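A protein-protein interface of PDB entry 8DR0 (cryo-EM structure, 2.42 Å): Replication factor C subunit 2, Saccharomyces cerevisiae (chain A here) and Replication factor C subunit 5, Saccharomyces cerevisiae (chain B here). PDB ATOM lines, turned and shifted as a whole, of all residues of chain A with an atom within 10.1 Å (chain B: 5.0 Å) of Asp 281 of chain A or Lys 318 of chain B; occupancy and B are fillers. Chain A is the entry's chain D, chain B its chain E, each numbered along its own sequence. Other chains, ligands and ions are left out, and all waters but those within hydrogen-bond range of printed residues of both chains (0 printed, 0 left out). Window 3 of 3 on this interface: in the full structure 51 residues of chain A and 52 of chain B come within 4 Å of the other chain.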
ATOM      1  N   LYS A 274      18.357   4.544 -26.554  1.00  0.00           N
ATOM      2  CA  LYS A 274      17.259   4.575 -25.595  1.00  0.00           C
ATOM      3  C   LYS A 274      17.722   4.106 -24.222  1.00  0.00           C
ATOM      4  O   LYS A 274      17.333   4.678 -23.197  1.00  0.00           O
ATOM      5  CB  LYS A 274      16.096   3.717 -26.091  1.00  0.00           C
ATOM      6  CG  LYS A 274      14.829   4.506 -26.378  1.00  0.00           C
ATOM      7  CD  LYS A 274      14.870   5.143 -27.757  1.00  0.00           C
ATOM      8  CE  LYS A 274      13.544   5.791 -28.112  1.00  0.00           C
ATOM      9  NZ  LYS A 274      13.081   6.733 -27.056  1.00  0.00           N
ATOM     10  N   VAL A 275      18.552   3.063 -24.182  1.00  0.00           N
ATOM     11  CA  VAL A 275      19.093   2.595 -22.909  1.00  0.00           C
ATOM     12  C   VAL A 275      19.959   3.676 -22.272  1.00  0.00           C
ATOM     13  O   VAL A 275      19.884   3.921 -21.063  1.00  0.00           O
ATOM     14  CB  VAL A 275      19.879   1.286 -23.116  1.00  0.00           C
ATOM     15  CG1 VAL A 275      20.731   0.975 -21.900  1.00  0.00           C
ATOM     16  CG2 VAL A 275      18.924   0.141 -23.410  1.00  0.00           C
ATOM     17  N   SER A 277      19.655   6.816 -22.574  1.00  0.00           N
ATOM     18  CA  SER A 277      18.810   7.890 -22.062  1.00  0.00           C
ATOM     19  C   SER A 277      18.399   7.625 -20.618  1.00  0.00           C
ATOM     20  O   SER A 277      18.409   8.539 -19.784  1.00  0.00           O
ATOM     21  CB  SER A 277      17.575   8.051 -22.948  1.00  0.00           C
ATOM     22  OG  SER A 277      16.478   7.320 -22.430  1.00  0.00           O
ATOM     23  N   GLY A 278      18.033   6.384 -20.304  1.00  0.00           N
ATOM     24  CA  GLY A 278      17.691   6.001 -18.951  1.00  0.00           C
ATOM     25  C   GLY A 278      16.252   6.238 -18.551  1.00  0.00           C
ATOM     26  O   GLY A 278      15.884   5.914 -17.415  1.00  0.00           O
ATOM     27  N   ASP A 279      15.425   6.787 -19.437  1.00  0.00           N
ATOM     28  CA  ASP A 279      14.028   7.058 -19.116  1.00  0.00           C
ATOM     29  C   ASP A 279      13.225   5.767 -19.229  1.00  0.00           C
ATOM     30  O   ASP A 279      13.228   5.118 -20.281  1.00  0.00           O
ATOM     31  CB  ASP A 279      13.473   8.133 -20.048  1.00  0.00           C
ATOM     32  CG  ASP A 279      12.055   8.544 -19.694  1.00  0.00           C
ATOM     33  OD1 ASP A 279      11.200   7.657 -19.493  1.00  0.00           O
ATOM     34  OD2 ASP A 279      11.795   9.763 -19.617  1.00  0.00           O
ATOM     35  N   PHE A 280      12.533   5.399 -18.149  1.00  0.00           N
ATOM     36  CA  PHE A 280      11.802   4.137 -18.131  1.00  0.00           C
ATOM     37  C   PHE A 280      10.670   4.136 -19.152  1.00  0.00           C
ATOM     38  O   PHE A 280      10.493   3.168 -19.900  1.00  0.00           O
ATOM     39  CB  PHE A 280      11.255   3.869 -16.727  1.00  0.00           C
ATOM     40  CG  PHE A 280      10.627   2.512 -16.569  1.00  0.00           C
ATOM     41  CD1 PHE A 280       9.338   2.272 -17.018  1.00  0.00           C
ATOM     42  CD2 PHE A 280      11.324   1.478 -15.971  1.00  0.00           C
ATOM     43  CE1 PHE A 280       8.760   1.025 -16.876  1.00  0.00           C
ATOM     44  CE2 PHE A 280      10.750   0.230 -15.824  1.00  0.00           C
ATOM     45  CZ  PHE A 280       9.468   0.003 -16.279  1.00  0.00           C
ATOM     46  N   ASP A 281       9.883   5.214 -19.191  1.00  0.00           N
ATOM     47  CA  ASP A 281       8.717   5.240 -20.067  1.00  0.00           C
ATOM     48  C   ASP A 281       9.122   5.175 -21.535  1.00  0.00           C
ATOM     49  O   ASP A 281       8.492   4.468 -22.330  1.00  0.00           O
ATOM     50  CB  ASP A 281       7.887   6.493 -19.796  1.00  0.00           C
ATOM     51  CG  ASP A 281       7.167   6.437 -18.464  1.00  0.00           C
ATOM     52  OD1 ASP A 281       6.997   7.501 -17.833  1.00  0.00           O
ATOM     53  OD2 ASP A 281       6.769   5.328 -18.047  1.00  0.00           O
ATOM     54  N   GLU A 282      10.163   5.918 -21.917  1.00  0.00           N
ATOM     55  CA  GLU A 282      10.608   5.895 -23.305  1.00  0.00           C
ATOM     56  C   GLU A 282      11.090   4.506 -23.700  1.00  0.00           C
ATOM     57  O   GLU A 282      10.770   4.013 -24.789  1.00  0.00           O
ATOM     58  CB  GLU A 282      11.715   6.928 -23.516  1.00  0.00           C
ATOM     59  CG  GLU A 282      11.224   8.367 -23.608  1.00  0.00           C
ATOM     60  CD  GLU A 282      10.228   8.582 -24.733  1.00  0.00           C
ATOM     61  OE1 GLU A 282      10.645   9.036 -25.819  1.00  0.00           O
ATOM     62  OE2 GLU A 282       9.028   8.302 -24.529  1.00  0.00           O
ATOM     63  N   ILE A 283      11.857   3.855 -22.822  1.00  0.00           N
ATOM     64  CA  ILE A 283      12.321   2.500 -23.101  1.00  0.00           C
ATOM     65  C   ILE A 283      11.135   1.557 -23.246  1.00  0.00           C
ATOM     66  O   ILE A 283      11.108   0.705 -24.140  1.00  0.00           O
ATOM     67  CB  ILE A 283      13.290   2.030 -22.001  1.00  0.00           C
ATOM     68  CG1 ILE A 283      14.592   2.832 -22.058  1.00  0.00           C
ATOM     69  CG2 ILE A 283      13.583   0.543 -22.145  1.00  0.00           C
ATOM     70  CD1 ILE A 283      15.361   2.838 -20.758  1.00  0.00           C
ATOM     71  N   LYS A 284      10.140   1.688 -22.366  1.00  0.00           N
ATOM     72  CA  LYS A 284       8.977   0.810 -22.431  1.00  0.00           C
ATOM     73  C   LYS A 284       8.225   0.989 -23.743  1.00  0.00           C
ATOM     74  O   LYS A 284       7.848   0.009 -24.395  1.00  0.00           O
ATOM     75  CB  LYS A 284       8.053   1.078 -21.243  1.00  0.00           C
ATOM     76  CG  LYS A 284       6.750   0.294 -21.289  1.00  0.00           C
ATOM     77  CD  LYS A 284       6.081   0.214 -19.926  1.00  0.00           C
ATOM     78  CE  LYS A 284       5.812   1.592 -19.339  1.00  0.00           C
ATOM     79  NZ  LYS A 284       4.935   2.416 -20.212  1.00  0.00           N
ATOM     80  N   LYS A 285       7.997   2.240 -24.152  1.00  0.00           N
ATOM     81  CA  LYS A 285       7.297   2.483 -25.410  1.00  0.00           C
ATOM     82  C   LYS A 285       8.089   1.943 -26.595  1.00  0.00           C
ATOM     83  O   LYS A 285       7.522   1.318 -27.504  1.00  0.00           O
ATOM     84  CB  LYS A 285       7.026   3.977 -25.591  1.00  0.00           C
ATOM     85  CG  LYS A 285       6.192   4.605 -24.488  1.00  0.00           C
ATOM     86  CD  LYS A 285       6.100   6.117 -24.660  1.00  0.00           C
ATOM     87  CE  LYS A 285       6.000   6.840 -23.325  1.00  0.00           C
ATOM     88  NZ  LYS A 285       7.267   7.540 -22.974  1.00  0.00           N
ATOM     89  N   TYR A 286       9.404   2.174 -26.605  1.00  0.00           N
ATOM     90  CA  TYR A 286      10.211   1.691 -27.717  1.00  0.00           C
ATOM     91  C   TYR A 286      10.196   0.171 -27.783  1.00  0.00           C
ATOM     92  O   TYR A 286      10.122  -0.404 -28.871  1.00  0.00           O
ATOM     93  CB  TYR A 286      11.646   2.202 -27.610  1.00  0.00           C
ATOM     94  CG  TYR A 286      12.454   1.899 -28.848  1.00  0.00           C
ATOM     95  CD1 TYR A 286      13.161   0.711 -28.967  1.00  0.00           C
ATOM     96  CD2 TYR A 286      12.489   2.790 -29.912  1.00  0.00           C
ATOM     97  CE1 TYR A 286      13.891   0.426 -30.101  1.00  0.00           C
ATOM     98  CE2 TYR A 286      13.217   2.513 -31.051  1.00  0.00           C
ATOM     99  CZ  TYR A 286      13.916   1.328 -31.141  1.00  0.00           C
ATOM    100  OH  TYR A 286      14.642   1.048 -32.274  1.00  0.00           O
ATOM    101  N   VAL A 287      10.273  -0.500 -26.632  1.00  0.00           N
ATOM    102  CA  VAL A 287      10.246  -1.958 -26.630  1.00  0.00           C
ATOM    103  C   VAL A 287       8.880  -2.465 -27.079  1.00  0.00           C
ATOM    104  O   VAL A 287       8.781  -3.480 -27.778  1.00  0.00           O
ATOM    105  CB  VAL A 287      10.627  -2.498 -25.240  1.00  0.00           C
ATOM    106  CG1 VAL A 287      10.463  -4.009 -25.191  1.00  0.00           C
ATOM    107  CG2 VAL A 287      12.056  -2.117 -24.899  1.00  0.00           C
ATOM    108  N   ASN A 288       7.808  -1.778 -26.681  1.00  0.00           N
ATOM    109  CA  ASN A 288       6.481  -2.177 -27.136  1.00  0.00           C
ATOM    110  C   ASN A 288       6.382  -2.096 -28.652  1.00  0.00           C
ATOM    111  O   ASN A 288       5.837  -2.999 -29.297  1.00  0.00           O
ATOM    112  CB  ASN A 288       5.414  -1.299 -26.483  1.00  0.00           C
ATOM    113  CG  ASN A 288       4.008  -1.701 -26.882  1.00  0.00           C
ATOM    114  OD1 ASN A 288       3.447  -2.657 -26.348  1.00  0.00           O
ATOM    115  ND2 ASN A 288       3.431  -0.974 -27.830  1.00  0.00           N
ATOM    116  N   THR A 289       6.903  -1.018 -29.240  1.00  0.00           N
ATOM    117  CA  THR A 289       6.917  -0.919 -30.698  1.00  0.00           C
ATOM    118  C   THR A 289       7.821  -1.983 -31.315  1.00  0.00           C
ATOM    119  O   THR A 289       7.491  -2.562 -32.355  1.00  0.00           O
ATOM    120  CB  THR A 289       7.366   0.478 -31.125  1.00  0.00           C
ATOM    121  OG1 THR A 289       6.437   1.453 -30.634  1.00  0.00           O
ATOM    122  CG2 THR A 289       7.440   0.580 -32.642  1.00  0.00           C
ATOM    123  N   HIS A 340       8.897 -10.484 -24.214  1.00  0.00           N
ATOM    124  CA  HIS A 340       8.688  -9.056 -23.987  1.00  0.00           C
ATOM    125  C   HIS A 340       9.132  -8.652 -22.584  1.00  0.00           C
ATOM    126  O   HIS A 340       9.901  -7.697 -22.411  1.00  0.00           O
ATOM    127  CB  HIS A 340       7.212  -8.721 -24.212  1.00  0.00           C
ATOM    128  CG  HIS A 340       6.916  -7.255 -24.286  1.00  0.00           C
ATOM    129  ND1 HIS A 340       7.816  -6.286 -23.901  1.00  0.00           N
ATOM    130  CD2 HIS A 340       5.809  -6.595 -24.701  1.00  0.00           C
ATOM    131  CE1 HIS A 340       7.277  -5.092 -24.074  1.00  0.00           C
ATOM    132  NE2 HIS A 340       6.059  -5.252 -24.560  1.00  0.00           N
ATOM    133  N   ILE A 341       8.661  -9.379 -21.568  1.00  0.00           N
ATOM    134  CA  ILE A 341       8.962  -9.021 -20.184  1.00  0.00           C
ATOM    135  C   ILE A 341      10.459  -9.119 -19.922  1.00  0.00           C
ATOM    136  O   ILE A 341      11.063  -8.226 -19.314  1.00  0.00           O
ATOM    137  CB  ILE A 341       8.161  -9.915 -19.219  1.00  0.00           C
ATOM    138  CG1 ILE A 341       6.682  -9.525 -19.239  1.00  0.00           C
ATOM    139  CG2 ILE A 341       8.720  -9.817 -17.806  1.00  0.00           C
ATOM    140  CD1 ILE A 341       5.758 -10.606 -18.720  1.00  0.00           C
ATOM    141  N   LEU A 344      12.391  -6.285 -21.688  1.00  0.00           N
ATOM    142  CA  LEU A 344      12.194  -5.006 -21.015  1.00  0.00           C
ATOM    143  C   LEU A 344      12.981  -4.947 -19.711  1.00  0.00           C
ATOM    144  O   LEU A 344      13.614  -3.930 -19.404  1.00  0.00           O
ATOM    145  CB  LEU A 344      10.706  -4.770 -20.754  1.00  0.00           C
ATOM    146  CG  LEU A 344      10.351  -3.424 -20.114  1.00  0.00           C
ATOM    147  CD1 LEU A 344      10.861  -2.266 -20.959  1.00  0.00           C
ATOM    148  CD2 LEU A 344       8.852  -3.309 -19.898  1.00  0.00           C
ATOM    149  N   ASN A 345      12.955  -6.032 -18.932  1.00  0.00           N
ATOM    150  CA  ASN A 345      13.707  -6.056 -17.682  1.00  0.00           C
ATOM    151  C   ASN A 345      15.199  -5.896 -17.938  1.00  0.00           C
ATOM    152  O   ASN A 345      15.877  -5.124 -17.247  1.00  0.00           O
ATOM    153  CB  ASN A 345      13.429  -7.358 -16.932  1.00  0.00           C
ATOM    154  CG  ASN A 345      14.234  -7.479 -15.654  1.00  0.00           C
ATOM    155  OD1 ASN A 345      14.191  -6.601 -14.794  1.00  0.00           O
ATOM    156  ND2 ASN A 345      14.975  -8.572 -15.525  1.00  0.00           N
ATOM    157  N   VAL A 348      15.965  -2.242 -18.959  1.00  0.00           N
ATOM    158  CA  VAL A 348      15.875  -1.328 -17.823  1.00  0.00           C
ATOM    159  C   VAL A 348      17.086  -1.491 -16.913  1.00  0.00           C
ATOM    160  O   VAL A 348      17.694  -0.503 -16.473  1.00  0.00           O
ATOM    161  CB  VAL A 348      14.556  -1.559 -17.061  1.00  0.00           C
ATOM    162  CG1 VAL A 348      14.605  -0.903 -15.688  1.00  0.00           C
ATOM    163  CG2 VAL A 348      13.381  -1.034 -17.868  1.00  0.00           C
ATOM    164  N   LYS A 349      17.463  -2.738 -16.620  1.00  0.00           N
ATOM    165  CA  LYS A 349      18.598  -2.970 -15.734  1.00  0.00           C
ATOM    166  C   LYS A 349      19.889  -2.433 -16.338  1.00  0.00           C
ATOM    167  O   LYS A 349      20.719  -1.859 -15.623  1.00  0.00           O
ATOM    168  CB  LYS A 349      18.722  -4.460 -15.420  1.00  0.00           C
ATOM    169  CG  LYS A 349      17.690  -4.949 -14.418  1.00  0.00           C
ATOM    170  CD  LYS A 349      17.802  -6.440 -14.169  1.00  0.00           C
ATOM    171  CE  LYS A 349      17.260  -6.811 -12.801  1.00  0.00           C
ATOM    172  NZ  LYS A 349      18.155  -6.359 -11.702  1.00  0.00           N
ATOM    173  N   SER A 351      20.037   0.087 -18.434  1.00  0.00           N
ATOM    174  CA  SER A 351      19.904   1.536 -18.362  1.00  0.00           C
ATOM    175  C   SER A 351      20.215   2.073 -16.973  1.00  0.00           C
ATOM    176  O   SER A 351      20.656   3.220 -16.850  1.00  0.00           O
ATOM    177  CB  SER A 351      18.491   1.953 -18.771  1.00  0.00           C
ATOM    178  OG  SER A 351      17.645   2.062 -17.639  1.00  0.00           O
ATOM    179  N   GLN A 352      19.998   1.279 -15.927  1.00  0.00           N
ATOM    180  CA  GLN A 352      20.297   1.710 -14.569  1.00  0.00           C
ATOM    181  C   GLN A 352      21.740   1.444 -14.157  1.00  0.00           C
ATOM    182  O   GLN A 352      22.108   1.748 -13.019  1.00  0.00           O
ATOM    183  CB  GLN A 352      19.344   1.037 -13.578  1.00  0.00           C
ATOM    184  CG  GLN A 352      17.987   1.714 -13.494  1.00  0.00           C
ATOM    185  CD  GLN A 352      16.910   0.804 -12.943  1.00  0.00           C
ATOM    186  OE1 GLN A 352      17.201  -0.248 -12.374  1.00  0.00           O
ATOM    187  NE2 GLN A 352      15.657   1.209 -13.105  1.00  0.00           N
ATOM    188  N   LEU B 308       2.535  -1.048 -15.037  1.00  0.00           N
ATOM    189  CA  LEU B 308       3.565  -0.145 -15.535  1.00  0.00           C
ATOM    190  C   LEU B 308       2.980   1.113 -16.166  1.00  0.00           C
ATOM    191  O   LEU B 308       3.688   2.118 -16.278  1.00  0.00           O
ATOM    192  CB  LEU B 308       4.458  -0.868 -16.545  1.00  0.00           C
ATOM    193  CG  LEU B 308       5.360  -1.965 -15.972  1.00  0.00           C
ATOM    194  CD1 LEU B 308       6.081  -2.697 -17.092  1.00  0.00           C
ATOM    195  CD2 LEU B 308       6.356  -1.393 -14.976  1.00  0.00           C
ATOM    196  N   VAL B 310       0.512   2.810 -14.816  1.00  0.00           N
ATOM    197  CA  VAL B 310      -0.018   3.670 -13.766  1.00  0.00           C
ATOM    198  C   VAL B 310       0.854   4.912 -13.641  1.00  0.00           C
ATOM    199  O   VAL B 310       2.086   4.843 -13.741  1.00  0.00           O
ATOM    200  CB  VAL B 310      -0.098   2.902 -12.436  1.00  0.00           C
ATOM    201  CG1 VAL B 310      -0.522   3.831 -11.309  1.00  0.00           C
ATOM    202  CG2 VAL B 310      -1.060   1.731 -12.557  1.00  0.00           C
ATOM    203  N   LEU B 313       2.971   5.702  -9.871  1.00  0.00           N
ATOM    204  CA  LEU B 313       4.198   4.985  -9.556  1.00  0.00           C
ATOM    205  C   LEU B 313       5.417   5.726 -10.093  1.00  0.00           C
ATOM    206  O   LEU B 313       5.363   6.391 -11.130  1.00  0.00           O
ATOM    207  CB  LEU B 313       4.149   3.572 -10.140  1.00  0.00           C
ATOM    208  CG  LEU B 313       2.898   2.752  -9.818  1.00  0.00           C
ATOM    209  CD1 LEU B 313       3.095   1.301 -10.226  1.00  0.00           C
ATOM    210  CD2 LEU B 313       2.544   2.851  -8.343  1.00  0.00           C
ATOM    211  N   ASN B 314       6.527   5.603  -9.369  1.00  0.00           N
ATOM    212  CA  ASN B 314       7.789   6.212  -9.754  1.00  0.00           C
ATOM    213  C   ASN B 314       8.678   5.177 -10.445  1.00  0.00           C
ATOM    214  O   ASN B 314       8.300   4.020 -10.640  1.00  0.00           O
ATOM    215  CB  ASN B 314       8.485   6.819  -8.534  1.00  0.00           C
ATOM    216  CG  ASN B 314       8.800   5.792  -7.464  1.00  0.00           C
ATOM    217  OD1 ASN B 314       9.453   4.782  -7.727  1.00  0.00           O
ATOM    218  ND2 ASN B 314       8.343   6.049  -6.245  1.00  0.00           N
ATOM    219  N   THR B 315       9.884   5.609 -10.818  1.00  0.00           N
ATOM    220  CA  THR B 315      10.783   4.739 -11.574  1.00  0.00           C
ATOM    221  C   THR B 315      11.183   3.510 -10.767  1.00  0.00           C
ATOM    222  O   THR B 315      11.245   2.399 -11.306  1.00  0.00           O
ATOM    223  CB  THR B 315      12.023   5.521 -12.006  1.00  0.00           C
ATOM    224  OG1 THR B 315      11.626   6.755 -12.615  1.00  0.00           O
ATOM    225  CG2 THR B 315      12.848   4.714 -12.998  1.00  0.00           C
ATOM    226  N   THR B 316      11.468   3.690  -9.474  1.00  0.00           N
ATOM    227  CA  THR B 316      11.884   2.559  -8.648  1.00  0.00           C
ATOM    228  C   THR B 316      10.788   1.505  -8.561  1.00  0.00           C
ATOM    229  O   THR B 316      11.059   0.302  -8.677  1.00  0.00           O
ATOM    230  CB  THR B 316      12.264   3.047  -7.249  1.00  0.00           C
ATOM    231  OG1 THR B 316      12.968   4.291  -7.348  1.00  0.00           O
ATOM    232  CG2 THR B 316      13.141   2.025  -6.545  1.00  0.00           C
ATOM    233  N   ASN B 317       9.542   1.938  -8.355  1.00  0.00           N
ATOM    234  CA  ASN B 317       8.437   0.992  -8.265  1.00  0.00           C
ATOM    235  C   ASN B 317       8.279   0.212  -9.563  1.00  0.00           C
ATOM    236  O   ASN B 317       8.079  -1.007  -9.542  1.00  0.00           O
ATOM    237  CB  ASN B 317       7.142   1.731  -7.927  1.00  0.00           C
ATOM    238  CG  ASN B 317       7.210   2.448  -6.595  1.00  0.00           C
ATOM    239  OD1 ASN B 317       7.951   2.048  -5.698  1.00  0.00           O
ATOM    240  ND2 ASN B 317       6.435   3.517  -6.458  1.00  0.00           N
ATOM    241  N   LYS B 318       8.365   0.898 -10.703  1.00  0.00           N
ATOM    242  CA  LYS B 318       8.222   0.222 -11.988  1.00  0.00           C
ATOM    243  C   LYS B 318       9.364  -0.761 -12.232  1.00  0.00           C
ATOM    244  O   LYS B 318       9.142  -1.864 -12.747  1.00  0.00           O
ATOM    245  CB  LYS B 318       8.141   1.260 -13.107  1.00  0.00           C
ATOM    246  CG  LYS B 318       6.730   1.770 -13.360  1.00  0.00           C
ATOM    247  CD  LYS B 318       6.684   3.280 -13.532  1.00  0.00           C
ATOM    248  CE  LYS B 318       7.463   3.739 -14.750  1.00  0.00           C
ATOM    249  NZ  LYS B 318       7.370   5.212 -14.942  1.00  0.00           N
ATOM    250  N   SER B 319      10.592  -0.378 -11.872  1.00  0.00           N
ATOM    251  CA  SER B 319      11.724  -1.287 -12.025  1.00  0.00           C
ATOM    252  C   SER B 319      11.531  -2.541 -11.180  1.00  0.00           C
ATOM    253  O   SER B 319      11.744  -3.667 -11.650  1.00  0.00           O
ATOM    254  CB  SER B 319      13.019  -0.572 -11.639  1.00  0.00           C
ATOM    255  OG  SER B 319      13.240   0.560 -12.462  1.00  0.00           O
ATOM    256  N   SER B 320      11.115  -2.362  -9.924  1.00  0.00           N
ATOM    257  CA  SER B 320      10.859  -3.514  -9.066  1.00  0.00           C
ATOM    258  C   SER B 320       9.744  -4.380  -9.638  1.00  0.00           C
ATOM    259  O   SER B 320       9.828  -5.615  -9.610  1.00  0.00           O
ATOM    260  CB  SER B 320      10.506  -3.046  -7.655  1.00  0.00           C
ATOM    261  OG  SER B 320      11.566  -2.303  -7.086  1.00  0.00           O
ATOM    262  N   ILE B 321       8.694  -3.747 -10.165  1.00  0.00           N
ATOM    263  CA  ILE B 321       7.566  -4.495 -10.712  1.00  0.00           C
ATOM    264  C   ILE B 321       8.020  -5.354 -11.883  1.00  0.00           C
ATOM    265  O   ILE B 321       7.660  -6.530 -11.986  1.00  0.00           O
ATOM    266  CB  ILE B 321       6.438  -3.532 -11.122  1.00  0.00           C
ATOM    267  CG1 ILE B 321       5.729  -2.984  -9.884  1.00  0.00           C
ATOM    268  CG2 ILE B 321       5.439  -4.232 -12.036  1.00  0.00           C
ATOM    269  CD1 ILE B 321       5.017  -1.670 -10.123  1.00  0.00           C
ATOM    270  N   ILE B 322       8.816  -4.780 -12.788  1.00  0.00           N
ATOM    271  CA  ILE B 322       9.240  -5.537 -13.963  1.00  0.00           C
ATOM    272  C   ILE B 322      10.193  -6.659 -13.561  1.00  0.00           C
ATOM    273  O   ILE B 322      10.143  -7.763 -14.122  1.00  0.00           O
ATOM    274  CB  ILE B 322       9.857  -4.599 -15.021  1.00  0.00           C
ATOM    275  CG1 ILE B 322      10.156  -5.363 -16.316  1.00  0.00           C
ATOM    276  CG2 ILE B 322      11.117  -3.931 -14.502  1.00  0.00           C
ATOM    277  CD1 ILE B 322       8.922  -5.878 -17.025  1.00  0.00           C
ATOM    278  N   GLU B 323      11.066  -6.411 -12.580  1.00  0.00           N
ATOM    279  CA  GLU B 323      11.950  -7.475 -12.106  1.00  0.00           C
ATOM    280  C   GLU B 323      11.147  -8.636 -11.523  1.00  0.00           C
ATOM    281  O   GLU B 323      11.395  -9.810 -11.843  1.00  0.00           O
ATOM    282  CB  GLU B 323      12.924  -6.916 -11.069  1.00  0.00           C
ATOM    283  CG  GLU B 323      14.123  -7.809 -10.801  1.00  0.00           C
ATOM    284  CD  GLU B 323      14.979  -7.305  -9.656  1.00  0.00           C
ATOM    285  OE1 GLU B 323      14.417  -6.987  -8.587  1.00  0.00           O
ATOM    286  OE2 GLU B 323      16.213  -7.228  -9.823  1.00  0.00           O
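NE2 of Gln 352 of chain A sits at hydrogen-bond distance from OG of Ser 319 of chain B (2.6 Å).
The side-chain amino group (NZ) of Lys 349 of chain A is in salt-bridge range of the side-chain carboxylate (OE2) of Glu 323 of chain B (2.8 Å).
The side-chain carboxylate (OD2) of Asp 281 of chain A lies within salt-bridge range of the side-chain amino group (NZ) of Lys 318 of chain B, at 3.2 Å.
The backbone carbonyl oxygen of Thr 315 of chain B is in hydrogen-bond range of the side-chain hydroxyl of Ser 319 of chain B, 2.9 Å away.
The side-chain amino group of Lys 285 of chain A lies close to the backbone carbonyl oxygen of Asp 281 of chain A.
The backbone carbonyl oxygen (O) of Val 348 of chain A sits at hydrogen-bond distance from the side-chain hydroxyl (OG) of Ser 351 of chain A (2.8 Å).
The backbone NH of Asp 281 of chain A is in hydrogen-bond range of the side-chain carboxylate of Asp 279 of chain A (2.8 Å).
Phe 280 of chain A touches Leu 308 of chain B (CZ to CD2, 3.7 Å).
Phe 280 of chain A touches Lys 318 of chain B (CD1 to CE, 3.3 Å).
CE of Lys 284 of chain A touches O of Leu 308 of chain B, at 3.8 Å.
O of Ile 341 of chain A touches CD1 of Ile 322 of chain B, 3.9 Å away.
Leu 308 of chain B touches Leu 344 of chain A.
CD1 of Ile 322 of chain B touches CD2 of Leu 344 of chain A (3.9 Å).
Ile 322 of chain B touches Asn 345 of chain A (CG1 to CA, 3.9 Å).
Asn 345 of chain A touches Glu 323 of chain B (OD1 to CA, 3.6 Å).
Val 348 of chain A touches Ser 319 of chain B.
Printed residues of chain B within 4 Å of Phe 280 of chain A: Leu 308 (3.7 Å) and Lys 318 (3.3 Å).
Of chain B, only Lys 318 comes within 4 Å of Asp 281 of chain A.
Ile 283 of chain A touches none of the printed residues of chain B.
Asn 288 of chain A touches none of the printed residues of chain B.
Of the printed residues of chain B, Ile 341 of chain A touches Ile 322.
Printed residues of chain B within 4 Å of Val 348 of chain A: Ser 319.
Thr 315 of chain B touches none of the printed residues of chain A.
No residue of chain A comes within 4 Å of Asn 317 of chain B.
Printed residues of chain A within 4 Å of Lys 318 of chain B: Phe 280 (3.3 Å) and Asp 281 (3.2 Å).
Of the printed residues of chain A, Ser 319 of chain B touches Val 348 (3.8 Å) and Gln 352 (2.6 Å).
Ser 320 of chain B touches none of the printed residues of chain A.
No residue of chain A comes within 4 Å of Ile 321 of chain B.
Printed residues of chain A within 4 Å of Glu 323 of chain B: Asn 345 and Lys 349.
The nearest residue of chain B that does not touch Asp 281 of chain A is Leu 308 of chain B (4.8 Å).
Of the 13 printed residues of chain B, 5 touch a printed residue of chain A.
Hydrophobic or aromatic side chains of chain B that line the printed part of chain A: Leu 308 and Ile 322.
Hydrophobic or aromatic side chains of chain A within 4 Å of the printed part of chain B: Phe 280, Leu 344 and Val 348.
Among the printed residues, Asp or Glu carboxylates within 4 Å of a Lys or Arg side-chain nitrogen of the other chain: Asp 281 of chain A with Lys 318 of chain B (3.2 Å) and Lys 349 of chain A with Glu 323 of chain B (2.8 Å).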
